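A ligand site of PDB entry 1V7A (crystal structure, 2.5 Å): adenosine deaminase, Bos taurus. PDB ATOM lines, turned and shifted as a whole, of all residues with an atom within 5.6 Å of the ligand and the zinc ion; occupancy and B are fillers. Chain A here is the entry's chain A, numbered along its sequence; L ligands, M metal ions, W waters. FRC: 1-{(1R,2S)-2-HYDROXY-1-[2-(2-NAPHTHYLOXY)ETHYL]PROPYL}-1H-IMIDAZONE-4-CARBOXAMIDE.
Water W1 bridges NE2 of His 237 (2.6 Å) and OD2 of Asp 294 (2.7 Å). Water W3 bridges an oxygen (O9) of the ligand (2.7 Å) and the backbone NH (N) of Gly 183 (2.8 Å). Water W4 bridges the side-chain carboxylate of Glu 216 and an oxygen (O9) of the ligand. Water W2 lies within hydrogen-bond range of OD1 of Asp 294 (2.9 Å), OE2 of Glu 216 (2.9 Å) and N10 of the ligand (3.3 Å). Water W5 lies within hydrogen-bond range of O of Ser 102 (2.7 Å), OD1 of Asp 18 (2.8 Å) and O15 of the ligand (3.5 Å).
O15 of the ligand sits at hydrogen-bond distance from ND1 of His 16, 3.1 Å away. An oxygen (O15) of the ligand lies within hydrogen-bond range of the side-chain carboxylate (OD2) of Asp 18 (2.7 Å). The side-chain carboxylate (OD1) of Asp 295 sits at hydrogen-bond distance from a nitrogen (N4) of the ligand, at 2.7 Å.
Phe 60 touches the ligand (CZ to N10, 3.7 Å). CD2 of Leu 61 touches C4 of the ligand, at 3.5 Å. CZ of Phe 64 touches C3 of the ligand, 3.3 Å away. Arg 100 touches the ligand (O to O15, 3.98 Å). Tyr 101 touches the ligand. N of Ser 102 touches O15 of the ligand (3.6 Å). Leu 105 touches the ligand (CD1 to O1, 3.6 Å). Trp 116 touches the ligand. SG of Cys 152 touches C9 of the ligand, at 3.8 Å. Met 154 touches the ligand (CE to C16, 3.6 Å). Ala 182 touches the ligand. C of Gly 183 touches C11 of the ligand, at 3.5 Å. Asp 184 touches the ligand (N to C11, 3.2 Å). Hydrophobic or aromatic side chains that line the ligand: His 16, Phe 60, Leu 61, Phe 64, Tyr 101, Leu 105, Trp 116, Met 154 and Ala 182. 16 residues have an atom within 4 Å of the ligand: His 16, Asp 18, Phe 60, Leu 61, Phe 64, Arg 100, Tyr 101, Ser 102, Leu 105, Trp 116, Cys 152, Met 154, Ala 182, Gly 183, Asp 184 and Asp 295. The nearest printed residue that does not touch the ligand is Asp 294 (4.3 Å).
The backbone NH of His 16 lies within hydrogen-bond range of the backbone carbonyl oxygen of Asp 294. The backbone carbonyl oxygen (O) of His 14 lies within hydrogen-bond range of the backbone NH (N) of Asp 294 (3.1 Å). ND1 of His 14 sits at hydrogen-bond distance from NH1 of Arg 100. The backbone carbonyl oxygen (O) of Tyr 101 sits at hydrogen-bond distance from the backbone NH (N) of Cys 152 (2.8 Å). O of Leu 105 is in hydrogen-bond range of NE1 of Trp 116 (2.7 Å). The backbone NH (N) of Leu 105 sits at hydrogen-bond distance from the side-chain hydroxyl (OG) of Ser 102, 3.5 Å away. O of Arg 100 lies within hydrogen-bond range of N of Leu 17.
The zinc ion is bound by water W1 (2.0 Å), a ring nitrogen (NE2) of His 16 (2.0 Å), a ring nitrogen (NE2) of His 213 (2.1 Å) and a ring nitrogen (NE2) of His 14 (2.1 Å). The zinc ion has four donor atoms within binding distance. Slightly farther from the zinc ion lies OD2 of Asp 294 (2.7 Å).
Within 4 Å of the zinc ion: His 14, His 16, His 213 and Asp 294. Along chain A the residues within 4 Å of the zinc ion span positions 14 to 294. The nearest printed residue that does not touch the zinc ion is His 237 (4.3 Å).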
ATOM      1  N   HIS A  14     -14.994 -25.215  13.854  1.00  0.00           N
ATOM      2  CA  HIS A  14     -16.227 -25.025  14.660  1.00  0.00           C
ATOM      3  C   HIS A  14     -17.070 -26.298  14.844  1.00  0.00           C
ATOM      4  O   HIS A  14     -18.070 -26.549  14.178  1.00  0.00           O
ATOM      5  CB  HIS A  14     -17.139 -23.934  14.081  1.00  0.00           C
ATOM      6  CG  HIS A  14     -18.150 -23.420  15.116  1.00  0.00           C
ATOM      7  ND1 HIS A  14     -18.152 -22.170  15.588  1.00  0.00           N
ATOM      8  CD2 HIS A  14     -19.140 -24.119  15.792  1.00  0.00           C
ATOM      9  CE1 HIS A  14     -19.107 -22.060  16.520  1.00  0.00           C
ATOM     10  NE2 HIS A  14     -19.722 -23.285  16.685  1.00  0.00           N
ATOM     11  N   HIS A  16     -18.061 -28.785  18.575  1.00  0.00           N
ATOM     12  CA  HIS A  16     -17.875 -28.937  20.029  1.00  0.00           C
ATOM     13  C   HIS A  16     -17.679 -30.400  20.445  1.00  0.00           C
ATOM     14  O   HIS A  16     -18.505 -31.228  20.107  1.00  0.00           O
ATOM     15  CB  HIS A  16     -19.086 -28.411  20.816  1.00  0.00           C
ATOM     16  CG  HIS A  16     -19.450 -26.950  20.556  1.00  0.00           C
ATOM     17  ND1 HIS A  16     -19.444 -25.979  21.498  1.00  0.00           N
ATOM     18  CD2 HIS A  16     -19.974 -26.391  19.389  1.00  0.00           C
ATOM     19  CE1 HIS A  16     -19.945 -24.855  20.961  1.00  0.00           C
ATOM     20  NE2 HIS A  16     -20.274 -25.095  19.648  1.00  0.00           N
ATOM     21  N   LEU A  17     -16.604 -30.672  21.216  1.00  0.00           N
ATOM     22  CA  LEU A  17     -16.279 -32.033  21.733  1.00  0.00           C
ATOM     23  C   LEU A  17     -17.411 -32.826  22.385  1.00  0.00           C
ATOM     24  O   LEU A  17     -17.788 -33.933  22.058  1.00  0.00           O
ATOM     25  CB  LEU A  17     -15.086 -31.892  22.690  1.00  0.00           C
ATOM     26  CG  LEU A  17     -14.633 -33.101  23.534  1.00  0.00           C
ATOM     27  CD1 LEU A  17     -14.338 -34.424  22.804  1.00  0.00           C
ATOM     28  CD2 LEU A  17     -13.349 -32.711  24.192  1.00  0.00           C
ATOM     29  N   ASP A  18     -17.995 -32.086  23.308  1.00  0.00           N
ATOM     30  CA  ASP A  18     -19.222 -32.459  24.018  1.00  0.00           C
ATOM     31  C   ASP A  18     -20.552 -32.367  23.268  1.00  0.00           C
ATOM     32  O   ASP A  18     -21.601 -32.826  23.686  1.00  0.00           O
ATOM     33  CB  ASP A  18     -19.247 -31.682  25.330  1.00  0.00           C
ATOM     34  CG  ASP A  18     -19.290 -30.167  25.128  1.00  0.00           C
ATOM     35  OD1 ASP A  18     -19.651 -29.515  26.101  1.00  0.00           O
ATOM     36  OD2 ASP A  18     -19.002 -29.644  24.056  1.00  0.00           O
ATOM     37  N   GLY A  19     -20.457 -31.763  22.083  1.00  0.00           N
ATOM     38  CA  GLY A  19     -21.481 -32.053  21.090  1.00  0.00           C
ATOM     39  C   GLY A  19     -21.132 -33.169  20.073  1.00  0.00           C
ATOM     40  O   GLY A  19     -21.816 -33.352  19.070  1.00  0.00           O
ATOM     41  N   LEU A  57     -34.750 -22.589  23.936  1.00  0.00           N
ATOM     42  CA  LEU A  57     -33.473 -22.735  24.658  1.00  0.00           C
ATOM     43  C   LEU A  57     -33.507 -23.715  25.868  1.00  0.00           C
ATOM     44  O   LEU A  57     -32.749 -24.668  25.890  1.00  0.00           O
ATOM     45  CB  LEU A  57     -32.898 -21.288  24.876  1.00  0.00           C
ATOM     46  CG  LEU A  57     -31.466 -21.102  25.419  1.00  0.00           C
ATOM     47  CD1 LEU A  57     -31.153 -19.636  25.628  1.00  0.00           C
ATOM     48  CD2 LEU A  57     -31.187 -21.763  26.752  1.00  0.00           C
ATOM     49  N   PHE A  60     -33.589 -27.141  24.456  1.00  0.00           N
ATOM     50  CA  PHE A  60     -32.174 -27.386  24.002  1.00  0.00           C
ATOM     51  C   PHE A  60     -31.086 -27.599  25.063  1.00  0.00           C
ATOM     52  O   PHE A  60     -30.168 -28.395  24.893  1.00  0.00           O
ATOM     53  CB  PHE A  60     -31.712 -26.291  23.001  1.00  0.00           C
ATOM     54  CG  PHE A  60     -30.229 -26.310  22.576  1.00  0.00           C
ATOM     55  CD1 PHE A  60     -29.842 -26.998  21.412  1.00  0.00           C
ATOM     56  CD2 PHE A  60     -29.255 -25.587  23.309  1.00  0.00           C
ATOM     57  CE1 PHE A  60     -28.505 -26.985  20.966  1.00  0.00           C
ATOM     58  CE2 PHE A  60     -27.915 -25.566  22.875  1.00  0.00           C
ATOM     59  CZ  PHE A  60     -27.549 -26.267  21.707  1.00  0.00           C
ATOM     60  N   LEU A  61     -31.181 -26.853  26.176  1.00  0.00           N
ATOM     61  CA  LEU A  61     -30.149 -27.123  27.176  1.00  0.00           C
ATOM     62  C   LEU A  61     -30.397 -28.331  28.044  1.00  0.00           C
ATOM     63  O   LEU A  61     -29.519 -28.971  28.610  1.00  0.00           O
ATOM     64  CB  LEU A  61     -29.937 -26.017  28.184  1.00  0.00           C
ATOM     65  CG  LEU A  61     -29.650 -24.643  27.612  1.00  0.00           C
ATOM     66  CD1 LEU A  61     -29.430 -23.715  28.812  1.00  0.00           C
ATOM     67  CD2 LEU A  61     -28.555 -24.657  26.579  1.00  0.00           C
ATOM     68  N   PHE A  64     -28.153 -31.297  27.158  1.00  0.00           N
ATOM     69  CA  PHE A  64     -26.822 -31.322  27.783  1.00  0.00           C
ATOM     70  C   PHE A  64     -26.915 -31.831  29.236  1.00  0.00           C
ATOM     71  O   PHE A  64     -26.153 -32.689  29.674  1.00  0.00           O
ATOM     72  CB  PHE A  64     -26.128 -29.962  27.682  1.00  0.00           C
ATOM     73  CG  PHE A  64     -25.700 -29.532  26.279  1.00  0.00           C
ATOM     74  CD1 PHE A  64     -26.471 -28.556  25.604  1.00  0.00           C
ATOM     75  CD2 PHE A  64     -24.520 -30.049  25.703  1.00  0.00           C
ATOM     76  CE1 PHE A  64     -25.999 -28.023  24.392  1.00  0.00           C
ATOM     77  CE2 PHE A  64     -24.061 -29.544  24.470  1.00  0.00           C
ATOM     78  CZ  PHE A  64     -24.790 -28.503  23.854  1.00  0.00           C
ATOM     79  N   MET A  68     -24.253 -35.003  29.431  1.00  0.00           N
ATOM     80  CA  MET A  68     -23.006 -34.552  30.073  1.00  0.00           C
ATOM     81  C   MET A  68     -22.581 -35.216  31.399  1.00  0.00           C
ATOM     82  O   MET A  68     -21.423 -35.572  31.550  1.00  0.00           O
ATOM     83  CB  MET A  68     -23.017 -33.048  30.231  1.00  0.00           C
ATOM     84  CG  MET A  68     -22.942 -32.301  28.900  1.00  0.00           C
ATOM     85  SD  MET A  68     -21.350 -32.496  28.122  1.00  0.00           S
ATOM     86  CE  MET A  68     -20.446 -31.355  29.162  1.00  0.00           C
ATOM     87  N   ARG A 100     -13.481 -27.342  19.829  1.00  0.00           N
ATOM     88  CA  ARG A 100     -13.665 -26.520  21.026  1.00  0.00           C
ATOM     89  C   ARG A 100     -14.572 -27.137  22.062  1.00  0.00           C
ATOM     90  O   ARG A 100     -15.437 -27.982  21.799  1.00  0.00           O
ATOM     91  CB  ARG A 100     -14.273 -25.142  20.752  1.00  0.00           C
ATOM     92  CG  ARG A 100     -15.670 -25.235  20.128  1.00  0.00           C
ATOM     93  CD  ARG A 100     -15.586 -24.802  18.678  1.00  0.00           C
ATOM     94  NE  ARG A 100     -15.803 -23.368  18.690  1.00  0.00           N
ATOM     95  CZ  ARG A 100     -15.521 -22.545  17.710  1.00  0.00           C
ATOM     96  NH1 ARG A 100     -16.371 -21.547  17.618  1.00  0.00           N
ATOM     97  NH2 ARG A 100     -14.519 -22.625  16.851  1.00  0.00           N
ATOM     98  N   TYR A 101     -14.324 -26.626  23.261  1.00  0.00           N
ATOM     99  CA  TYR A 101     -15.106 -27.063  24.414  1.00  0.00           C
ATOM    100  C   TYR A 101     -14.831 -26.197  25.642  1.00  0.00           C
ATOM    101  O   TYR A 101     -13.794 -25.561  25.788  1.00  0.00           O
ATOM    102  CB  TYR A 101     -14.853 -28.568  24.679  1.00  0.00           C
ATOM    103  CG  TYR A 101     -13.442 -28.793  25.168  1.00  0.00           C
ATOM    104  CD1 TYR A 101     -13.271 -28.805  26.563  1.00  0.00           C
ATOM    105  CD2 TYR A 101     -12.369 -28.928  24.250  1.00  0.00           C
ATOM    106  CE1 TYR A 101     -11.965 -28.871  27.057  1.00  0.00           C
ATOM    107  CE2 TYR A 101     -11.062 -29.033  24.770  1.00  0.00           C
ATOM    108  CZ  TYR A 101     -10.877 -28.971  26.172  1.00  0.00           C
ATOM    109  OH  TYR A 101      -9.622 -29.015  26.742  1.00  0.00           O
ATOM    110  N   SER A 102     -15.776 -26.273  26.569  1.00  0.00           N
ATOM    111  CA  SER A 102     -15.506 -25.781  27.925  1.00  0.00           C
ATOM    112  C   SER A 102     -15.032 -26.808  28.963  1.00  0.00           C
ATOM    113  O   SER A 102     -15.693 -27.801  29.285  1.00  0.00           O
ATOM    114  CB  SER A 102     -16.778 -25.090  28.421  1.00  0.00           C
ATOM    115  OG  SER A 102     -16.638 -24.766  29.802  1.00  0.00           O
ATOM    116  N   LEU A 105     -17.109 -27.247  32.165  1.00  0.00           N
ATOM    117  CA  LEU A 105     -18.262 -28.148  31.985  1.00  0.00           C
ATOM    118  C   LEU A 105     -17.961 -29.648  31.814  1.00  0.00           C
ATOM    119  O   LEU A 105     -18.808 -30.520  31.696  1.00  0.00           O
ATOM    120  CB  LEU A 105     -19.135 -27.600  30.850  1.00  0.00           C
ATOM    121  CG  LEU A 105     -19.634 -26.170  31.066  1.00  0.00           C
ATOM    122  CD1 LEU A 105     -20.480 -25.691  29.893  1.00  0.00           C
ATOM    123  CD2 LEU A 105     -20.455 -26.053  32.364  1.00  0.00           C
ATOM    124  N   TRP A 116     -24.062 -29.610  36.009  1.00  0.00           N
ATOM    125  CA  TRP A 116     -24.772 -30.856  35.659  1.00  0.00           C
ATOM    126  C   TRP A 116     -25.416 -31.593  36.809  1.00  0.00           C
ATOM    127  O   TRP A 116     -25.449 -32.828  36.862  1.00  0.00           O
ATOM    128  CB  TRP A 116     -23.912 -31.846  34.866  1.00  0.00           C
ATOM    129  CG  TRP A 116     -23.128 -31.165  33.781  1.00  0.00           C
ATOM    130  CD1 TRP A 116     -21.731 -31.163  33.679  1.00  0.00           C
ATOM    131  CD2 TRP A 116     -23.620 -30.365  32.676  1.00  0.00           C
ATOM    132  NE1 TRP A 116     -21.339 -30.435  32.624  1.00  0.00           N
ATOM    133  CE2 TRP A 116     -22.449 -29.909  31.976  1.00  0.00           C
ATOM    134  CE3 TRP A 116     -24.910 -29.982  32.233  1.00  0.00           C
ATOM    135  CZ2 TRP A 116     -22.593 -29.063  30.858  1.00  0.00           C
ATOM    136  CZ3 TRP A 116     -25.035 -29.140  31.104  1.00  0.00           C
ATOM    137  CH2 TRP A 116     -23.885 -28.677  30.439  1.00  0.00           C
ATOM    138  N   CYS A 152     -13.321 -22.804  25.786  1.00  0.00           N
ATOM    139  CA  CYS A 152     -14.497 -21.902  25.744  1.00  0.00           C
ATOM    140  C   CYS A 152     -14.869 -21.215  27.038  1.00  0.00           C
ATOM    141  O   CYS A 152     -15.414 -21.850  27.926  1.00  0.00           O
ATOM    142  CB  CYS A 152     -15.772 -22.618  25.353  1.00  0.00           C
ATOM    143  SG  CYS A 152     -15.855 -23.343  23.674  1.00  0.00           S
ATOM    144  N   MET A 154     -17.760 -19.265  29.048  1.00  0.00           N
ATOM    145  CA  MET A 154     -19.203 -19.213  28.818  1.00  0.00           C
ATOM    146  C   MET A 154     -19.800 -17.840  29.132  1.00  0.00           C
ATOM    147  O   MET A 154     -19.431 -17.179  30.101  1.00  0.00           O
ATOM    148  CB  MET A 154     -19.915 -20.269  29.704  1.00  0.00           C
ATOM    149  CG  MET A 154     -19.515 -21.725  29.478  1.00  0.00           C
ATOM    150  SD  MET A 154     -19.821 -22.319  27.825  1.00  0.00           S
ATOM    151  CE  MET A 154     -21.590 -22.322  28.064  1.00  0.00           C
ATOM    152  N   HIS A 156     -22.713 -16.639  30.192  1.00  0.00           N
ATOM    153  CA  HIS A 156     -23.306 -16.380  31.510  1.00  0.00           C
ATOM    154  C   HIS A 156     -22.339 -16.493  32.699  1.00  0.00           C
ATOM    155  O   HIS A 156     -22.713 -16.337  33.849  1.00  0.00           O
ATOM    156  CB  HIS A 156     -24.524 -17.262  31.745  1.00  0.00           C
ATOM    157  CG  HIS A 156     -24.048 -18.670  32.037  1.00  0.00           C
ATOM    158  ND1 HIS A 156     -23.516 -19.477  31.129  1.00  0.00           N
ATOM    159  CD2 HIS A 156     -23.994 -19.303  33.276  1.00  0.00           C
ATOM    160  CE1 HIS A 156     -23.102 -20.608  31.745  1.00  0.00           C
ATOM    161  NE2 HIS A 156     -23.399 -20.508  33.074  1.00  0.00           N
ATOM    162  N   ALA A 182     -18.752 -18.817  24.435  1.00  0.00           N
ATOM    163  CA  ALA A 182     -19.865 -19.662  24.084  1.00  0.00           C
ATOM    164  C   ALA A 182     -21.004 -19.676  25.077  1.00  0.00           C
ATOM    165  O   ALA A 182     -20.918 -19.243  26.221  1.00  0.00           O
ATOM    166  CB  ALA A 182     -19.422 -21.089  23.748  1.00  0.00           C
ATOM    167  N   GLY A 183     -22.083 -20.213  24.514  1.00  0.00           N
ATOM    168  CA  GLY A 183     -23.425 -20.348  25.089  1.00  0.00           C
ATOM    169  C   GLY A 183     -24.214 -19.071  25.394  1.00  0.00           C
ATOM    170  O   GLY A 183     -23.879 -18.362  26.321  1.00  0.00           O
ATOM    171  N   ASP A 184     -25.251 -18.772  24.551  1.00  0.00           N
ATOM    172  CA  ASP A 184     -26.177 -17.704  24.912  1.00  0.00           C
ATOM    173  C   ASP A 184     -25.714 -16.229  24.884  1.00  0.00           C
ATOM    174  O   ASP A 184     -25.824 -15.417  25.789  1.00  0.00           O
ATOM    175  CB  ASP A 184     -26.973 -17.979  26.193  1.00  0.00           C
ATOM    176  CG  ASP A 184     -28.255 -17.171  26.304  1.00  0.00           C
ATOM    177  OD1 ASP A 184     -28.650 -16.505  25.364  1.00  0.00           O
ATOM    178  OD2 ASP A 184     -28.843 -17.230  27.367  1.00  0.00           O
ATOM    179  N   HIS A 213     -18.570 -16.878  19.607  1.00  0.00           N
ATOM    180  CA  HIS A 213     -19.882 -17.116  18.992  1.00  0.00           C
ATOM    181  C   HIS A 213     -20.799 -16.082  18.313  1.00  0.00           C
ATOM    182  O   HIS A 213     -21.265 -16.387  17.254  1.00  0.00           O
ATOM    183  CB  HIS A 213     -20.754 -18.073  19.798  1.00  0.00           C
ATOM    184  CG  HIS A 213     -20.363 -19.511  19.615  1.00  0.00           C
ATOM    185  ND1 HIS A 213     -19.192 -19.954  20.007  1.00  0.00           N
ATOM    186  CD2 HIS A 213     -21.108 -20.601  19.174  1.00  0.00           C
ATOM    187  CE1 HIS A 213     -19.163 -21.306  19.845  1.00  0.00           C
ATOM    188  NE2 HIS A 213     -20.360 -21.747  19.315  1.00  0.00           N
ATOM    189  N   GLU A 216     -25.181 -16.133  15.543  1.00  0.00           N
ATOM    190  CA  GLU A 216     -26.194 -17.173  15.275  1.00  0.00           C
ATOM    191  C   GLU A 216     -27.616 -16.835  15.727  1.00  0.00           C
ATOM    192  O   GLU A 216     -28.580 -17.051  15.037  1.00  0.00           O
ATOM    193  CB  GLU A 216     -25.703 -18.441  15.939  1.00  0.00           C
ATOM    194  CG  GLU A 216     -26.692 -19.573  16.203  1.00  0.00           C
ATOM    195  CD  GLU A 216     -25.979 -20.565  17.087  1.00  0.00           C
ATOM    196  OE1 GLU A 216     -25.467 -20.159  18.118  1.00  0.00           O
ATOM    197  OE2 GLU A 216     -25.920 -21.749  16.758  1.00  0.00           O
ATOM    198  N   HIS A 237     -20.344 -18.759  13.533  1.00  0.00           N
ATOM    199  CA  HIS A 237     -21.575 -18.411  12.800  1.00  0.00           C
ATOM    200  C   HIS A 237     -21.593 -17.025  12.173  1.00  0.00           C
ATOM    201  O   HIS A 237     -21.483 -16.856  10.969  1.00  0.00           O
ATOM    202  CB  HIS A 237     -22.909 -18.516  13.536  1.00  0.00           C
ATOM    203  CG  HIS A 237     -23.095 -19.861  14.221  1.00  0.00           C
ATOM    204  ND1 HIS A 237     -23.830 -20.866  13.711  1.00  0.00           N
ATOM    205  CD2 HIS A 237     -22.594 -20.252  15.453  1.00  0.00           C
ATOM    206  CE1 HIS A 237     -23.808 -21.902  14.561  1.00  0.00           C
ATOM    207  NE2 HIS A 237     -23.057 -21.490  15.616  1.00  0.00           N
ATOM    208  N   ASP A 294     -20.714 -28.134  13.954  1.00  0.00           N
ATOM    209  CA  ASP A 294     -21.169 -27.701  15.267  1.00  0.00           C
ATOM    210  C   ASP A 294     -21.312 -28.745  16.373  1.00  0.00           C
ATOM    211  O   ASP A 294     -20.576 -28.726  17.352  1.00  0.00           O
ATOM    212  CB  ASP A 294     -22.409 -26.876  15.085  1.00  0.00           C
ATOM    213  CG  ASP A 294     -22.536 -25.746  16.046  1.00  0.00           C
ATOM    214  OD1 ASP A 294     -23.505 -25.015  15.887  1.00  0.00           O
ATOM    215  OD2 ASP A 294     -21.697 -25.599  16.937  1.00  0.00           O
ATOM    216  N   ASP A 295     -22.321 -29.618  16.226  1.00  0.00           N
ATOM    217  CA  ASP A 295     -22.623 -30.673  17.230  1.00  0.00           C
ATOM    218  C   ASP A 295     -23.280 -31.921  16.623  1.00  0.00           C
ATOM    219  O   ASP A 295     -24.506 -32.020  16.584  1.00  0.00           O
ATOM    220  CB  ASP A 295     -23.654 -30.195  18.270  1.00  0.00           C
ATOM    221  CG  ASP A 295     -23.305 -28.886  18.946  1.00  0.00           C
ATOM    222  OD1 ASP A 295     -22.788 -28.932  20.051  1.00  0.00           O
ATOM    223  OD2 ASP A 295     -23.583 -27.837  18.370  1.00  0.00           O
ATOM    224  N   PHE A 299     -27.183 -32.716  16.473  1.00  0.00           N
ATOM    225  CA  PHE A 299     -27.832 -32.434  15.195  1.00  0.00           C
ATOM    226  C   PHE A 299     -28.024 -33.671  14.290  1.00  0.00           C
ATOM    227  O   PHE A 299     -28.381 -33.568  13.123  1.00  0.00           O
ATOM    228  CB  PHE A 299     -27.081 -31.274  14.489  1.00  0.00           C
ATOM    229  CG  PHE A 299     -27.032 -30.013  15.325  1.00  0.00           C
ATOM    230  CD1 PHE A 299     -28.168 -29.502  15.991  1.00  0.00           C
ATOM    231  CD2 PHE A 299     -25.800 -29.315  15.415  1.00  0.00           C
ATOM    232  CE1 PHE A 299     -28.108 -28.286  16.698  1.00  0.00           C
ATOM    233  CE2 PHE A 299     -25.726 -28.098  16.127  1.00  0.00           C
ATOM    234  CZ  PHE A 299     -26.887 -27.593  16.759  1.00  0.00           C
HETATM  235  C1  FRC L   1     -22.151 -25.323  23.470  1.00  0.00           C
HETATM  236  N2  FRC L   1     -21.470 -26.512  23.981  1.00  0.00           N
HETATM  237  C3  FRC L   1     -21.708 -27.526  23.152  1.00  0.00           C
HETATM  238  N4  FRC L   1     -22.381 -27.111  22.060  1.00  0.00           N
HETATM  239  C5  FRC L   1     -22.777 -25.716  22.353  1.00  0.00           C
HETATM  240  C8  FRC L   1     -23.741 -24.913  21.565  1.00  0.00           C
HETATM  241  O9  FRC L   1     -24.085 -23.789  21.883  1.00  0.00           O
HETATM  242  N10 FRC L   1     -24.202 -25.464  20.446  1.00  0.00           N
HETATM  243  C13 FRC L   1     -20.751 -26.615  25.233  1.00  0.00           C
HETATM  244  C14 FRC L   1     -19.286 -26.143  25.079  1.00  0.00           C
HETATM  245  O15 FRC L   1     -18.430 -26.990  24.223  1.00  0.00           O
HETATM  246  C18 FRC L   1     -21.509 -25.962  26.390  1.00  0.00           C
HETATM  247  C2  FRC L   1     -22.618 -26.912  26.864  1.00  0.00           C
HETATM  248  C9  FRC L   1     -19.248 -24.602  24.874  1.00  0.00           C
HETATM  249  O1  FRC L   1     -23.386 -26.331  27.899  1.00  0.00           O
HETATM  250  C11 FRC L   1     -26.795 -21.358  25.717  1.00  0.00           C
HETATM  251  C17 FRC L   1     -26.414 -21.746  27.013  1.00  0.00           C
HETATM  252  C12 FRC L   1     -25.596 -22.856  27.181  1.00  0.00           C
HETATM  253  C4  FRC L   1     -25.234 -23.647  26.068  1.00  0.00           C
HETATM  254  C15 FRC L   1     -25.603 -23.248  24.779  1.00  0.00           C
HETATM  255  C6  FRC L   1     -26.399 -22.111  24.605  1.00  0.00           C
HETATM  256  C7  FRC L   1     -25.254 -23.253  28.484  1.00  0.00           C
HETATM  257  C16 FRC L   1     -24.495 -24.413  28.639  1.00  0.00           C
HETATM  258  C19 FRC L   1     -24.110 -25.206  27.548  1.00  0.00           C
HETATM  259  C10 FRC L   1     -24.466 -24.809  26.240  1.00  0.00           C
HETATM  260 ZN    ZN M   1     -20.701 -23.587  18.468  1.00  0.00          ZN
HETATM  261  O   HOH W   1     -22.323 -23.050  17.517  1.00  0.00           O
HETATM  262  O   HOH W   2     -25.719 -24.505  17.689  1.00  0.00           O
HETATM  263  O   HOH W   3     -22.128 -22.079  22.489  1.00  0.00           O
HETATM  264  O   HOH W   4     -24.288 -21.749  19.895  1.00  0.00           O
HETATM  265  O   HOH W   5     -17.589 -28.179  27.395  1.00  0.00           O
